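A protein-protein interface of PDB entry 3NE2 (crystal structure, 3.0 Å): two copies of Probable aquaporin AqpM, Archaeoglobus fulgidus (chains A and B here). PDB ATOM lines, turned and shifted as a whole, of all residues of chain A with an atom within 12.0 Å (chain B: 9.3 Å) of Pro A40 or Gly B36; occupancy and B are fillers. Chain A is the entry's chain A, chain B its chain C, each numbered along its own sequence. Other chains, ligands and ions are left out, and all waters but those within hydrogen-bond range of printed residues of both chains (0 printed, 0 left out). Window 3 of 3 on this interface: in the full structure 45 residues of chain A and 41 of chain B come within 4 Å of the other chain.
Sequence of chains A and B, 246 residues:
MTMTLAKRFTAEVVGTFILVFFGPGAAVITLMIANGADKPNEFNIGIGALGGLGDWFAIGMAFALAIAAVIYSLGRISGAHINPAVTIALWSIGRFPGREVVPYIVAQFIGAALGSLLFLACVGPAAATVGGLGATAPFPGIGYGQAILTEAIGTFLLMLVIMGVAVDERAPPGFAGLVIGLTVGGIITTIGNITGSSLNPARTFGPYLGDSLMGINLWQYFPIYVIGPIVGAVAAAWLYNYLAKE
The backbone carbonyl oxygen (O) of Leu A50 sits close to the backbone carbonyl oxygen (O) of Leu B50, 2.8 Å away. OD1 of Asn A41 sits close to O of Ile B33 (3.4 Å). ND2 of Asn A44 sits at hydrogen-bond distance from O of Ile B33 (3.2 Å). The backbone carbonyl oxygen of Pro A40 lies close to the backbone carbonyl oxygen of Asn B35 (3.4 Å).
The side-chain amide oxygen of Asn A44 sits close to the backbone carbonyl oxygen of Ile A47. OD1 of Asn A41 sits at hydrogen-bond distance from N of Asn A44, at 3.4 Å. The backbone carbonyl oxygen (O) of Phe A43 lies close to the side-chain amide nitrogen (ND2) of Asn A193. The backbone NH (N) of Gly A46 sits at hydrogen-bond distance from the side-chain amide oxygen (OD1) of Asn A44, 2.9 Å away. N of Gly A48 lies within hydrogen-bond range of OD1 of Asp A55 (3.1 Å). The indole nitrogen (NE1) of Trp A56 lies within hydrogen-bond range of the side-chain amide oxygen (OD1) of Asn A193 (3.2 Å).
Among the printed residues, pairs that only touch across the chains: Pro A40 with Ile B33 (3.8 Å), Pro A40 with Gly B36 (3.9 Å), Pro A40 with Ala B37 (3.7 Å), Asn A41 with Met B32 (3.5 Å), Asn A41 with Asn B35 (3.5 Å), Phe A43 with Met B32 (3.6 Å), Phe A43 with Ile B33 (3.6 Å), Asn A44 with Leu B50 (3.8 Å), Gly A48 with Ile B33 (3.97 Å), Gly A48 with Leu B50 (3.2 Å), Ala A49 with Leu B50 (3.2 Å), Gly A51 with Leu B50 (3.97 Å), Gly A52 with Leu B50 (3.5 Å), Leu A53 with Thr B30 (3.0 Å) and Asn A193 with Ile B33 (3.5 Å).
Pro A40 touches four residues of chain B. Of the printed residues of chain B, Asn A41 touches Met B32 (3.5 Å), Ile B33 (3.4 Å) and Asn B35 (3.5 Å). Printed residues of chain A within 4 Å of Thr B30: Leu A53 (3.0 Å). No residue of chain A comes within 4 Å of Ala B34. Of chain A, only Pro A40 comes within 4 Å of Gly B36. Lys B39 touches none of the printed residues of chain A. The nearest residue of chain B that does not touch Pro A40 is Leu B50 (4.4 Å). The nearest residue of chain A that does not touch Gly B36 is Asn A41 (5.7 Å).
Hydrophobic or aromatic side chains of chain B that line the printed part of chain A: Met B32, Ile B33 and Leu B50. Printed residues of chain A that touch a printed residue of chain B: Pro A40, Asn A41, Phe A43, Asn A44, Gly A48, Ala A49, Leu A50, Gly A51, Gly A52, Leu A53 and Asn A193.
Ala A49 touches Leu B50, but with the chains exchanged Leu A50 does not touch Ala B49 (6.5 Å). Leu A50 touches its own counterpart, Leu B50. 11 positions are printed for both chains. Of the 19 pairs that touch across the chains among the printed residues, 1 has its exchanged pair printed and touching as well.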
ATOM      1  N   LEU A  31      35.351 -24.727  29.641  1.00  0.00           N
ATOM      2  CA  LEU A  31      33.995 -25.194  29.981  1.00  0.00           C
ATOM      3  C   LEU A  31      33.461 -24.679  31.356  1.00  0.00           C
ATOM      4  O   LEU A  31      32.285 -24.284  31.493  1.00  0.00           O
ATOM      5  CB  LEU A  31      33.950 -26.722  29.953  1.00  0.00           C
ATOM      6  CG  LEU A  31      33.902 -27.371  28.569  1.00  0.00           C
ATOM      7  CD1 LEU A  31      34.096 -28.909  28.629  1.00  0.00           C
ATOM      8  CD2 LEU A  31      32.590 -26.992  27.853  1.00  0.00           C
ATOM      9  N   ALA A  34      32.809 -20.836  31.186  1.00  0.00           N
ATOM     10  CA  ALA A  34      31.719 -20.619  30.237  1.00  0.00           C
ATOM     11  C   ALA A  34      30.427 -21.284  30.684  1.00  0.00           C
ATOM     12  O   ALA A  34      29.374 -21.049  30.088  1.00  0.00           O
ATOM     13  CB  ALA A  34      32.107 -21.144  28.862  1.00  0.00           C
ATOM     14  N   ASN A  35      30.496 -22.105  31.731  1.00  0.00           N
ATOM     15  CA  ASN A  35      29.332 -22.852  32.208  1.00  0.00           C
ATOM     16  C   ASN A  35      28.187 -21.938  32.632  1.00  0.00           C
ATOM     17  O   ASN A  35      28.293 -21.200  33.620  1.00  0.00           O
ATOM     18  CB  ASN A  35      29.716 -23.769  33.369  1.00  0.00           C
ATOM     19  CG  ASN A  35      28.535 -24.579  33.888  1.00  0.00           C
ATOM     20  OD1 ASN A  35      27.536 -24.804  33.178  1.00  0.00           O
ATOM     21  ND2 ASN A  35      28.643 -25.024  35.136  1.00  0.00           N
ATOM     22  N   GLY A  36      27.099 -22.014  31.869  1.00  0.00           N
ATOM     23  CA  GLY A  36      25.915 -21.208  32.117  1.00  0.00           C
ATOM     24  C   GLY A  36      25.574 -20.306  30.945  1.00  0.00           C
ATOM     25  O   GLY A  36      24.420 -19.898  30.794  1.00  0.00           O
ATOM     26  N   ALA A  37      26.561 -19.988  30.112  1.00  0.00           N
ATOM     27  CA  ALA A  37      26.334 -19.068  29.006  1.00  0.00           C
ATOM     28  C   ALA A  37      25.456 -19.688  27.916  1.00  0.00           C
ATOM     29  O   ALA A  37      25.408 -20.917  27.782  1.00  0.00           O
ATOM     30  CB  ALA A  37      27.650 -18.630  28.430  1.00  0.00           C
ATOM     31  N   ASP A  38      24.769 -18.823  27.157  1.00  0.00           N
ATOM     32  CA  ASP A  38      23.929 -19.232  26.023  1.00  0.00           C
ATOM     33  C   ASP A  38      24.710 -19.996  24.947  1.00  0.00           C
ATOM     34  O   ASP A  38      25.531 -19.417  24.243  1.00  0.00           O
ATOM     35  CB  ASP A  38      23.307 -18.009  25.337  1.00  0.00           C
ATOM     36  CG  ASP A  38      22.194 -17.364  26.150  1.00  0.00           C
ATOM     37  OD1 ASP A  38      21.485 -18.068  26.912  1.00  0.00           O
ATOM     38  OD2 ASP A  38      21.998 -16.133  26.007  1.00  0.00           O
ATOM     39  N   LYS A  39      24.452 -21.296  24.825  1.00  0.00           N
ATOM     40  CA  LYS A  39      24.975 -22.115  23.720  1.00  0.00           C
ATOM     41  C   LYS A  39      23.959 -22.099  22.569  1.00  0.00           C
ATOM     42  O   LYS A  39      22.962 -22.809  22.614  1.00  0.00           O
ATOM     43  CB  LYS A  39      25.236 -23.552  24.199  1.00  0.00           C
ATOM     44  CG  LYS A  39      26.140 -23.655  25.458  1.00  0.00           C
ATOM     45  CD  LYS A  39      26.394 -25.121  25.879  1.00  0.00           C
ATOM     46  CE  LYS A  39      25.107 -25.891  26.268  1.00  0.00           C
ATOM     47  NZ  LYS A  39      25.424 -27.233  26.862  1.00  0.00           N
ATOM     48  N   PRO A  40      24.227 -21.316  21.517  1.00  0.00           N
ATOM     49  CA  PRO A  40      23.234 -20.945  20.505  1.00  0.00           C
ATOM     50  C   PRO A  40      22.903 -22.033  19.491  1.00  0.00           C
ATOM     51  O   PRO A  40      22.075 -21.801  18.611  1.00  0.00           O
ATOM     52  CB  PRO A  40      23.920 -19.797  19.775  1.00  0.00           C
ATOM     53  CG  PRO A  40      25.349 -20.222  19.757  1.00  0.00           C
ATOM     54  CD  PRO A  40      25.587 -20.980  21.062  1.00  0.00           C
ATOM     55  N   ASN A  41      23.573 -23.181  19.576  1.00  0.00           N
ATOM     56  CA  ASN A  41      23.079 -24.395  18.930  1.00  0.00           C
ATOM     57  C   ASN A  41      23.675 -25.648  19.563  1.00  0.00           C
ATOM     58  O   ASN A  41      24.427 -25.545  20.525  1.00  0.00           O
ATOM     59  CB  ASN A  41      23.268 -24.362  17.405  1.00  0.00           C
ATOM     60  CG  ASN A  41      24.708 -24.625  16.970  1.00  0.00           C
ATOM     61  OD1 ASN A  41      25.664 -24.159  17.593  1.00  0.00           O
ATOM     62  ND2 ASN A  41      24.860 -25.361  15.873  1.00  0.00           N
ATOM     63  N   GLU A  42      23.291 -26.820  19.051  1.00  0.00           N
ATOM     64  CA  GLU A  42      23.710 -28.104  19.614  1.00  0.00           C
ATOM     65  C   GLU A  42      25.199 -28.315  19.422  1.00  0.00           C
ATOM     66  O   GLU A  42      25.888 -28.851  20.297  1.00  0.00           O
ATOM     67  CB  GLU A  42      22.946 -29.241  18.945  1.00  0.00           C
ATOM     68  CG  GLU A  42      23.283 -30.635  19.481  1.00  0.00           C
ATOM     69  CD  GLU A  42      22.244 -31.699  19.074  1.00  0.00           C
ATOM     70  OE1 GLU A  42      21.213 -31.358  18.419  1.00  0.00           O
ATOM     71  OE2 GLU A  42      22.459 -32.889  19.428  1.00  0.00           O
ATOM     72  N   PHE A  43      25.696 -27.878  18.271  1.00  0.00           N
ATOM     73  CA  PHE A  43      27.079 -28.121  17.900  1.00  0.00           C
ATOM     74  C   PHE A  43      28.020 -27.446  18.875  1.00  0.00           C
ATOM     75  O   PHE A  43      29.154 -27.923  19.052  1.00  0.00           O
ATOM     76  CB  PHE A  43      27.331 -27.632  16.467  1.00  0.00           C
ATOM     77  CG  PHE A  43      28.610 -28.161  15.836  1.00  0.00           C
ATOM     78  CD1 PHE A  43      29.544 -27.286  15.272  1.00  0.00           C
ATOM     79  CD2 PHE A  43      28.864 -29.536  15.775  1.00  0.00           C
ATOM     80  CE1 PHE A  43      30.706 -27.767  14.675  1.00  0.00           C
ATOM     81  CE2 PHE A  43      30.034 -30.024  15.179  1.00  0.00           C
ATOM     82  CZ  PHE A  43      30.953 -29.133  14.628  1.00  0.00           C
ATOM     83  N   ASN A  44      27.559 -26.331  19.469  1.00  0.00           N
ATOM     84  CA  ASN A  44      28.325 -25.586  20.476  1.00  0.00           C
ATOM     85  C   ASN A  44      28.060 -26.191  21.829  1.00  0.00           C
ATOM     86  O   ASN A  44      26.954 -26.123  22.313  1.00  0.00           O
ATOM     87  CB  ASN A  44      27.944 -24.095  20.477  1.00  0.00           C
ATOM     88  CG  ASN A  44      28.926 -23.229  21.273  1.00  0.00           C
ATOM     89  OD1 ASN A  44      29.241 -23.536  22.419  1.00  0.00           O
ATOM     90  ND2 ASN A  44      29.406 -22.135  20.660  1.00  0.00           N
ATOM     91  N   ILE A  45      29.081 -26.790  22.434  1.00  0.00           N
ATOM     92  CA  ILE A  45      28.921 -27.419  23.737  1.00  0.00           C
ATOM     93  C   ILE A  45      29.594 -26.632  24.851  1.00  0.00           C
ATOM     94  O   ILE A  45      29.949 -27.220  25.865  1.00  0.00           O
ATOM     95  CB  ILE A  45      29.505 -28.838  23.768  1.00  0.00           C
ATOM     96  CG1 ILE A  45      31.020 -28.781  23.665  1.00  0.00           C
ATOM     97  CG2 ILE A  45      28.881 -29.724  22.646  1.00  0.00           C
ATOM     98  CD1 ILE A  45      31.697 -29.646  24.688  1.00  0.00           C
ATOM     99  N   GLY A  46      29.791 -25.321  24.661  1.00  0.00           N
ATOM    100  CA  GLY A  46      30.264 -24.431  25.736  1.00  0.00           C
ATOM    101  C   GLY A  46      31.591 -23.815  25.425  1.00  0.00           C
ATOM    102  O   GLY A  46      31.850 -22.665  25.817  1.00  0.00           O
ATOM    103  N   ILE A  47      32.432 -24.592  24.734  1.00  0.00           N
ATOM    104  CA  ILE A  47      33.678 -24.083  24.132  1.00  0.00           C
ATOM    105  C   ILE A  47      33.300 -23.317  22.875  1.00  0.00           C
ATOM    106  O   ILE A  47      32.678 -23.881  21.954  1.00  0.00           O
ATOM    107  CB  ILE A  47      34.637 -25.226  23.800  1.00  0.00           C
ATOM    108  CG1 ILE A  47      35.175 -25.831  25.101  1.00  0.00           C
ATOM    109  CG2 ILE A  47      35.767 -24.720  22.908  1.00  0.00           C
ATOM    110  CD1 ILE A  47      35.837 -27.138  24.935  1.00  0.00           C
ATOM    111  N   GLY A  48      33.635 -22.027  22.859  1.00  0.00           N
ATOM    112  CA  GLY A  48      33.168 -21.106  21.811  1.00  0.00           C
ATOM    113  C   GLY A  48      32.002 -20.230  22.269  1.00  0.00           C
ATOM    114  O   GLY A  48      31.700 -19.209  21.649  1.00  0.00           O
ATOM    115  N   ALA A  49      31.346 -20.628  23.355  1.00  0.00           N
ATOM    116  CA  ALA A  49      30.188 -19.921  23.856  1.00  0.00           C
ATOM    117  C   ALA A  49      30.477 -18.444  24.129  1.00  0.00           C
ATOM    118  O   ALA A  49      29.706 -17.544  23.739  1.00  0.00           O
ATOM    119  CB  ALA A  49      29.710 -20.589  25.115  1.00  0.00           C
ATOM    120  N   LEU A  50      31.591 -18.201  24.803  1.00  0.00           N
ATOM    121  CA  LEU A  50      31.973 -16.844  25.183  1.00  0.00           C
ATOM    122  C   LEU A  50      33.010 -16.219  24.228  1.00  0.00           C
ATOM    123  O   LEU A  50      32.888 -15.051  23.849  1.00  0.00           O
ATOM    124  CB  LEU A  50      32.472 -16.836  26.636  1.00  0.00           C
ATOM    125  CG  LEU A  50      31.351 -17.022  27.682  1.00  0.00           C
ATOM    126  CD1 LEU A  50      31.883 -17.260  29.096  1.00  0.00           C
ATOM    127  CD2 LEU A  50      30.444 -15.814  27.675  1.00  0.00           C
ATOM    128  N   GLY A  51      34.007 -16.997  23.827  1.00  0.00           N
ATOM    129  CA  GLY A  51      35.095 -16.479  22.994  1.00  0.00           C
ATOM    130  C   GLY A  51      35.162 -17.019  21.577  1.00  0.00           C
ATOM    131  O   GLY A  51      36.189 -16.876  20.916  1.00  0.00           O
ATOM    132  N   GLY A  52      34.075 -17.640  21.116  1.00  0.00           N
ATOM    133  CA  GLY A  52      33.997 -18.201  19.759  1.00  0.00           C
ATOM    134  C   GLY A  52      35.131 -19.158  19.468  1.00  0.00           C
ATOM    135  O   GLY A  52      35.580 -19.850  20.363  1.00  0.00           O
ATOM    136  N   LEU A  53      35.606 -19.191  18.222  1.00  0.00           N
ATOM    137  CA  LEU A  53      36.712 -20.064  17.836  1.00  0.00           C
ATOM    138  C   LEU A  53      38.000 -19.668  18.562  1.00  0.00           C
ATOM    139  O   LEU A  53      38.935 -20.481  18.710  1.00  0.00           O
ATOM    140  CB  LEU A  53      36.935 -20.008  16.323  1.00  0.00           C
ATOM    141  CG  LEU A  53      37.776 -21.144  15.750  1.00  0.00           C
ATOM    142  CD1 LEU A  53      36.931 -22.416  15.621  1.00  0.00           C
ATOM    143  CD2 LEU A  53      38.380 -20.734  14.415  1.00  0.00           C
ATOM    144  N   ASP A  55      38.249 -19.353  21.619  1.00  0.00           N
ATOM    145  CA  ASP A  55      38.326 -20.322  22.714  1.00  0.00           C
ATOM    146  C   ASP A  55      39.142 -21.559  22.244  1.00  0.00           C
ATOM    147  O   ASP A  55      40.059 -22.017  22.935  1.00  0.00           O
ATOM    148  CB  ASP A  55      36.914 -20.724  23.222  1.00  0.00           C
ATOM    149  CG  ASP A  55      36.271 -19.668  24.115  1.00  0.00           C
ATOM    150  OD1 ASP A  55      35.027 -19.614  24.146  1.00  0.00           O
ATOM    151  OD2 ASP A  55      36.992 -18.894  24.778  1.00  0.00           O
ATOM    152  N   TRP A  56      38.822 -22.082  21.063  1.00  0.00           N
ATOM    153  CA  TRP A  56      39.547 -23.220  20.551  1.00  0.00           C
ATOM    154  C   TRP A  56      41.013 -22.904  20.325  1.00  0.00           C
ATOM    155  O   TRP A  56      41.846 -23.757  20.594  1.00  0.00           O
ATOM    156  CB  TRP A  56      38.911 -23.751  19.268  1.00  0.00           C
ATOM    157  CG  TRP A  56      37.867 -24.781  19.486  1.00  0.00           C
ATOM    158  CD1 TRP A  56      36.588 -24.734  19.036  1.00  0.00           C
ATOM    159  CD2 TRP A  56      38.002 -26.025  20.192  1.00  0.00           C
ATOM    160  NE1 TRP A  56      35.901 -25.867  19.416  1.00  0.00           N
ATOM    161  CE2 TRP A  56      36.749 -26.676  20.128  1.00  0.00           C
ATOM    162  CE3 TRP A  56      39.047 -26.648  20.872  1.00  0.00           C
ATOM    163  CZ2 TRP A  56      36.512 -27.934  20.728  1.00  0.00           C
ATOM    164  CZ3 TRP A  56      38.826 -27.897  21.454  1.00  0.00           C
ATOM    165  CH2 TRP A  56      37.569 -28.530  21.374  1.00  0.00           C
ATOM    166  N   PHE A 139      31.822 -35.078  18.198  1.00  0.00           N
ATOM    167  CA  PHE A 139      30.890 -33.975  18.467  1.00  0.00           C
ATOM    168  C   PHE A 139      29.540 -34.211  17.828  1.00  0.00           C
ATOM    169  O   PHE A 139      29.412 -35.070  16.973  1.00  0.00           O
ATOM    170  CB  PHE A 139      31.493 -32.629  18.040  1.00  0.00           C
ATOM    171  CG  PHE A 139      32.403 -32.033  19.079  1.00  0.00           C
ATOM    172  CD1 PHE A 139      33.587 -32.672  19.431  1.00  0.00           C
ATOM    173  CD2 PHE A 139      32.070 -30.863  19.726  1.00  0.00           C
ATOM    174  CE1 PHE A 139      34.422 -32.147  20.402  1.00  0.00           C
ATOM    175  CE2 PHE A 139      32.911 -30.332  20.706  1.00  0.00           C
ATOM    176  CZ  PHE A 139      34.085 -30.975  21.042  1.00  0.00           C
ATOM    177  N   PRO A 140      28.517 -33.474  18.275  1.00  0.00           N
ATOM    178  CA  PRO A 140      27.149 -33.600  17.737  1.00  0.00           C
ATOM    179  C   PRO A 140      27.053 -33.649  16.206  1.00  0.00           C
ATOM    180  O   PRO A 140      27.417 -32.689  15.514  1.00  0.00           O
ATOM    181  CB  PRO A 140      26.443 -32.359  18.265  1.00  0.00           C
ATOM    182  CG  PRO A 140      27.234 -31.965  19.518  1.00  0.00           C
ATOM    183  CD  PRO A 140      28.551 -32.690  19.523  1.00  0.00           C
ATOM    184  N   ASN A 193      36.467 -28.928  17.435  1.00  0.00           N
ATOM    185  CA  ASN A 193      35.038 -29.107  17.590  1.00  0.00           C
ATOM    186  C   ASN A 193      34.488 -30.249  16.749  1.00  0.00           C
ATOM    187  O   ASN A 193      33.272 -30.348  16.576  1.00  0.00           O
ATOM    188  CB  ASN A 193      34.304 -27.815  17.261  1.00  0.00           C
ATOM    189  CG  ASN A 193      33.021 -27.680  18.028  1.00  0.00           C
ATOM    190  OD1 ASN A 193      32.996 -27.036  19.070  1.00  0.00           O
ATOM    191  ND2 ASN A 193      31.942 -28.307  17.531  1.00  0.00           N
ATOM    192  N   THR B  30      34.105 -22.171  12.805  1.00  0.00           N
ATOM    193  CA  THR B  30      33.701 -20.911  13.419  1.00  0.00           C
ATOM    194  C   THR B  30      32.232 -20.692  13.138  1.00  0.00           C
ATOM    195  O   THR B  30      31.428 -20.531  14.067  1.00  0.00           O
ATOM    196  CB  THR B  30      34.446 -19.688  12.863  1.00  0.00           C
ATOM    197  OG1 THR B  30      35.857 -19.903  12.924  1.00  0.00           O
ATOM    198  CG2 THR B  30      34.083 -18.431  13.661  1.00  0.00           C
ATOM    199  N   LEU B  31      31.881 -20.693  11.853  1.00  0.00           N
ATOM    200  CA  LEU B  31      30.496 -20.421  11.438  1.00  0.00           C
ATOM    201  C   LEU B  31      29.514 -21.411  12.069  1.00  0.00           C
ATOM    202  O   LEU B  31      28.453 -21.022  12.574  1.00  0.00           O
ATOM    203  CB  LEU B  31      30.379 -20.432   9.908  1.00  0.00           C
ATOM    204  CG  LEU B  31      30.871 -19.160   9.216  1.00  0.00           C
ATOM    205  CD1 LEU B  31      30.949 -19.358   7.711  1.00  0.00           C
ATOM    206  CD2 LEU B  31      29.977 -17.958   9.584  1.00  0.00           C
ATOM    207  N   MET B  32      29.898 -22.685  12.056  1.00  0.00           N
ATOM    208  CA  MET B  32      29.052 -23.745  12.581  1.00  0.00           C
ATOM    209  C   MET B  32      28.800 -23.603  14.077  1.00  0.00           C
ATOM    210  O   MET B  32      27.660 -23.744  14.512  1.00  0.00           O
ATOM    211  CB  MET B  32      29.641 -25.127  12.270  1.00  0.00           C
ATOM    212  CG  MET B  32      29.356 -25.607  10.849  1.00  0.00           C
ATOM    213  SD  MET B  32      29.836 -27.323  10.556  1.00  0.00           S
ATOM    214  CE  MET B  32      28.732 -28.206  11.682  1.00  0.00           C
ATOM    215  N   ILE B  33      29.839 -23.333  14.868  1.00  0.00           N
ATOM    216  CA  ILE B  33      29.638 -23.236  16.317  1.00  0.00           C
ATOM    217  C   ILE B  33      28.927 -21.912  16.706  1.00  0.00           C
ATOM    218  O   ILE B  33      28.155 -21.844  17.686  1.00  0.00           O
ATOM    219  CB  ILE B  33      30.947 -23.488  17.116  1.00  0.00           C
ATOM    220  CG1 ILE B  33      31.922 -22.328  17.013  1.00  0.00           C
ATOM    221  CG2 ILE B  33      31.638 -24.740  16.620  1.00  0.00           C
ATOM    222  CD1 ILE B  33      32.986 -22.409  18.064  1.00  0.00           C
ATOM    223  N   ALA B  34      29.153 -20.881  15.895  1.00  0.00           N
ATOM    224  CA  ALA B  34      28.538 -19.569  16.121  1.00  0.00           C
ATOM    225  C   ALA B  34      27.165 -19.466  15.497  1.00  0.00           C
ATOM    226  O   ALA B  34      26.508 -18.450  15.654  1.00  0.00           O
ATOM    227  CB  ALA B  34      29.432 -18.465  15.556  1.00  0.00           C
ATOM    228  N   ASN B  35      26.747 -20.497  14.768  1.00  0.00           N
ATOM    229  CA  ASN B  35      25.449 -20.493  14.088  1.00  0.00           C
ATOM    230  C   ASN B  35      24.264 -20.388  15.058  1.00  0.00           C
ATOM    231  O   ASN B  35      23.986 -21.306  15.828  1.00  0.00           O
ATOM    232  CB  ASN B  35      25.281 -21.742  13.209  1.00  0.00           C
ATOM    233  CG  ASN B  35      23.910 -21.791  12.487  1.00  0.00           C
ATOM    234  OD1 ASN B  35      23.270 -20.759  12.250  1.00  0.00           O
ATOM    235  ND2 ASN B  35      23.470 -23.000  12.134  1.00  0.00           N
ATOM    236  N   GLY B  36      23.571 -19.258  14.991  1.00  0.00           N
ATOM    237  CA  GLY B  36      22.439 -18.985  15.859  1.00  0.00           C
ATOM    238  C   GLY B  36      22.635 -17.740  16.708  1.00  0.00           C
ATOM    239  O   GLY B  36      21.665 -17.109  17.112  1.00  0.00           O
ATOM    240  N   ALA B  37      23.888 -17.368  16.967  1.00  0.00           N
ATOM    241  CA  ALA B  37      24.180 -16.228  17.840  1.00  0.00           C
ATOM    242  C   ALA B  37      23.792 -14.897  17.189  1.00  0.00           C
ATOM    243  O   ALA B  37      23.709 -14.791  15.967  1.00  0.00           O
ATOM    244  CB  ALA B  37      25.635 -16.219  18.218  1.00  0.00           C
ATOM    245  N   ASP B  38      23.550 -13.890  18.024  1.00  0.00           N
ATOM    246  CA  ASP B  38      23.211 -12.534  17.563  1.00  0.00           C
ATOM    247  C   ASP B  38      24.304 -11.898  16.698  1.00  0.00           C
ATOM    248  O   ASP B  38      25.378 -11.561  17.197  1.00  0.00           O
ATOM    249  CB  ASP B  38      22.976 -11.614  18.767  1.00  0.00           C
ATOM    250  CG  ASP B  38      21.681 -11.904  19.491  1.00  0.00           C
ATOM    251  OD1 ASP B  38      20.701 -12.327  18.840  1.00  0.00           O
ATOM    252  OD2 ASP B  38      21.638 -11.685  20.720  1.00  0.00           O
ATOM    253  N   LYS B  39      24.029 -11.733  15.407  1.00  0.00           N
ATOM    254  CA  LYS B  39      24.899 -10.951  14.519  1.00  0.00           C
ATOM    255  C   LYS B  39      24.418  -9.485  14.543  1.00  0.00           C
ATOM    256  O   LYS B  39      23.411  -9.152  13.919  1.00  0.00           O
ATOM    257  CB  LYS B  39      24.894 -11.523  13.091  1.00  0.00           C
ATOM    258  N   ILE B  45      28.926 -11.588   9.644  1.00  0.00           N
ATOM    259  CA  ILE B  45      28.203 -12.734   9.094  1.00  0.00           C
ATOM    260  C   ILE B  45      28.352 -13.997   9.939  1.00  0.00           C
ATOM    261  O   ILE B  45      28.139 -15.099   9.437  1.00  0.00           O
ATOM    262  CB  ILE B  45      28.651 -13.053   7.648  1.00  0.00           C
ATOM    263  CG1 ILE B  45      30.115 -13.513   7.613  1.00  0.00           C
ATOM    264  CG2 ILE B  45      28.406 -11.842   6.742  1.00  0.00           C
ATOM    265  CD1 ILE B  45      30.346 -14.687   6.702  1.00  0.00           C
ATOM    266  N   GLY B  46      28.732 -13.845  11.206  1.00  0.00           N
ATOM    267  CA  GLY B  46      28.835 -14.985  12.128  1.00  0.00           C
ATOM    268  C   GLY B  46      30.237 -15.187  12.652  1.00  0.00           C
ATOM    269  O   GLY B  46      30.436 -15.565  13.808  1.00  0.00           O
ATOM    270  N   ALA B  49      30.966 -13.090  15.724  1.00  0.00           N
ATOM    271  CA  ALA B  49      29.738 -13.061  16.515  1.00  0.00           C
ATOM    272  C   ALA B  49      29.998 -13.387  17.978  1.00  0.00           C
ATOM    273  O   ALA B  49      29.526 -12.689  18.863  1.00  0.00           O
ATOM    274  CB  ALA B  49      28.736 -14.038  15.949  1.00  0.00           C
ATOM    275  N   LEU B  50      30.757 -14.460  18.222  1.00  0.00           N
ATOM    276  CA  LEU B  50      31.039 -14.935  19.590  1.00  0.00           C
ATOM    277  C   LEU B  50      32.401 -14.450  20.127  1.00  0.00           C
ATOM    278  O   LEU B  50      32.494 -14.015  21.289  1.00  0.00           O
ATOM    279  CB  LEU B  50      30.935 -16.474  19.650  1.00  0.00           C
ATOM    280  CG  LEU B  50      29.504 -17.014  19.584  1.00  0.00           C
ATOM    281  CD1 LEU B  50      29.446 -18.520  19.422  1.00  0.00           C
ATOM    282  CD2 LEU B  50      28.769 -16.583  20.841  1.00  0.00           C
ATOM    283  N   VAL B 130      26.136 -24.606   6.134  1.00  0.00           N
ATOM    284  CA  VAL B 130      26.334 -23.654   7.240  1.00  0.00           C
ATOM    285  C   VAL B 130      27.704 -23.000   7.225  1.00  0.00           C
ATOM    286  O   VAL B 130      27.829 -21.829   7.598  1.00  0.00           O
ATOM    287  CB  VAL B 130      26.151 -24.308   8.620  1.00  0.00           C
ATOM    288  CG1 VAL B 130      26.061 -23.234   9.702  1.00  0.00           C
ATOM    289  CG2 VAL B 130      24.907 -25.163   8.631  1.00  0.00           C
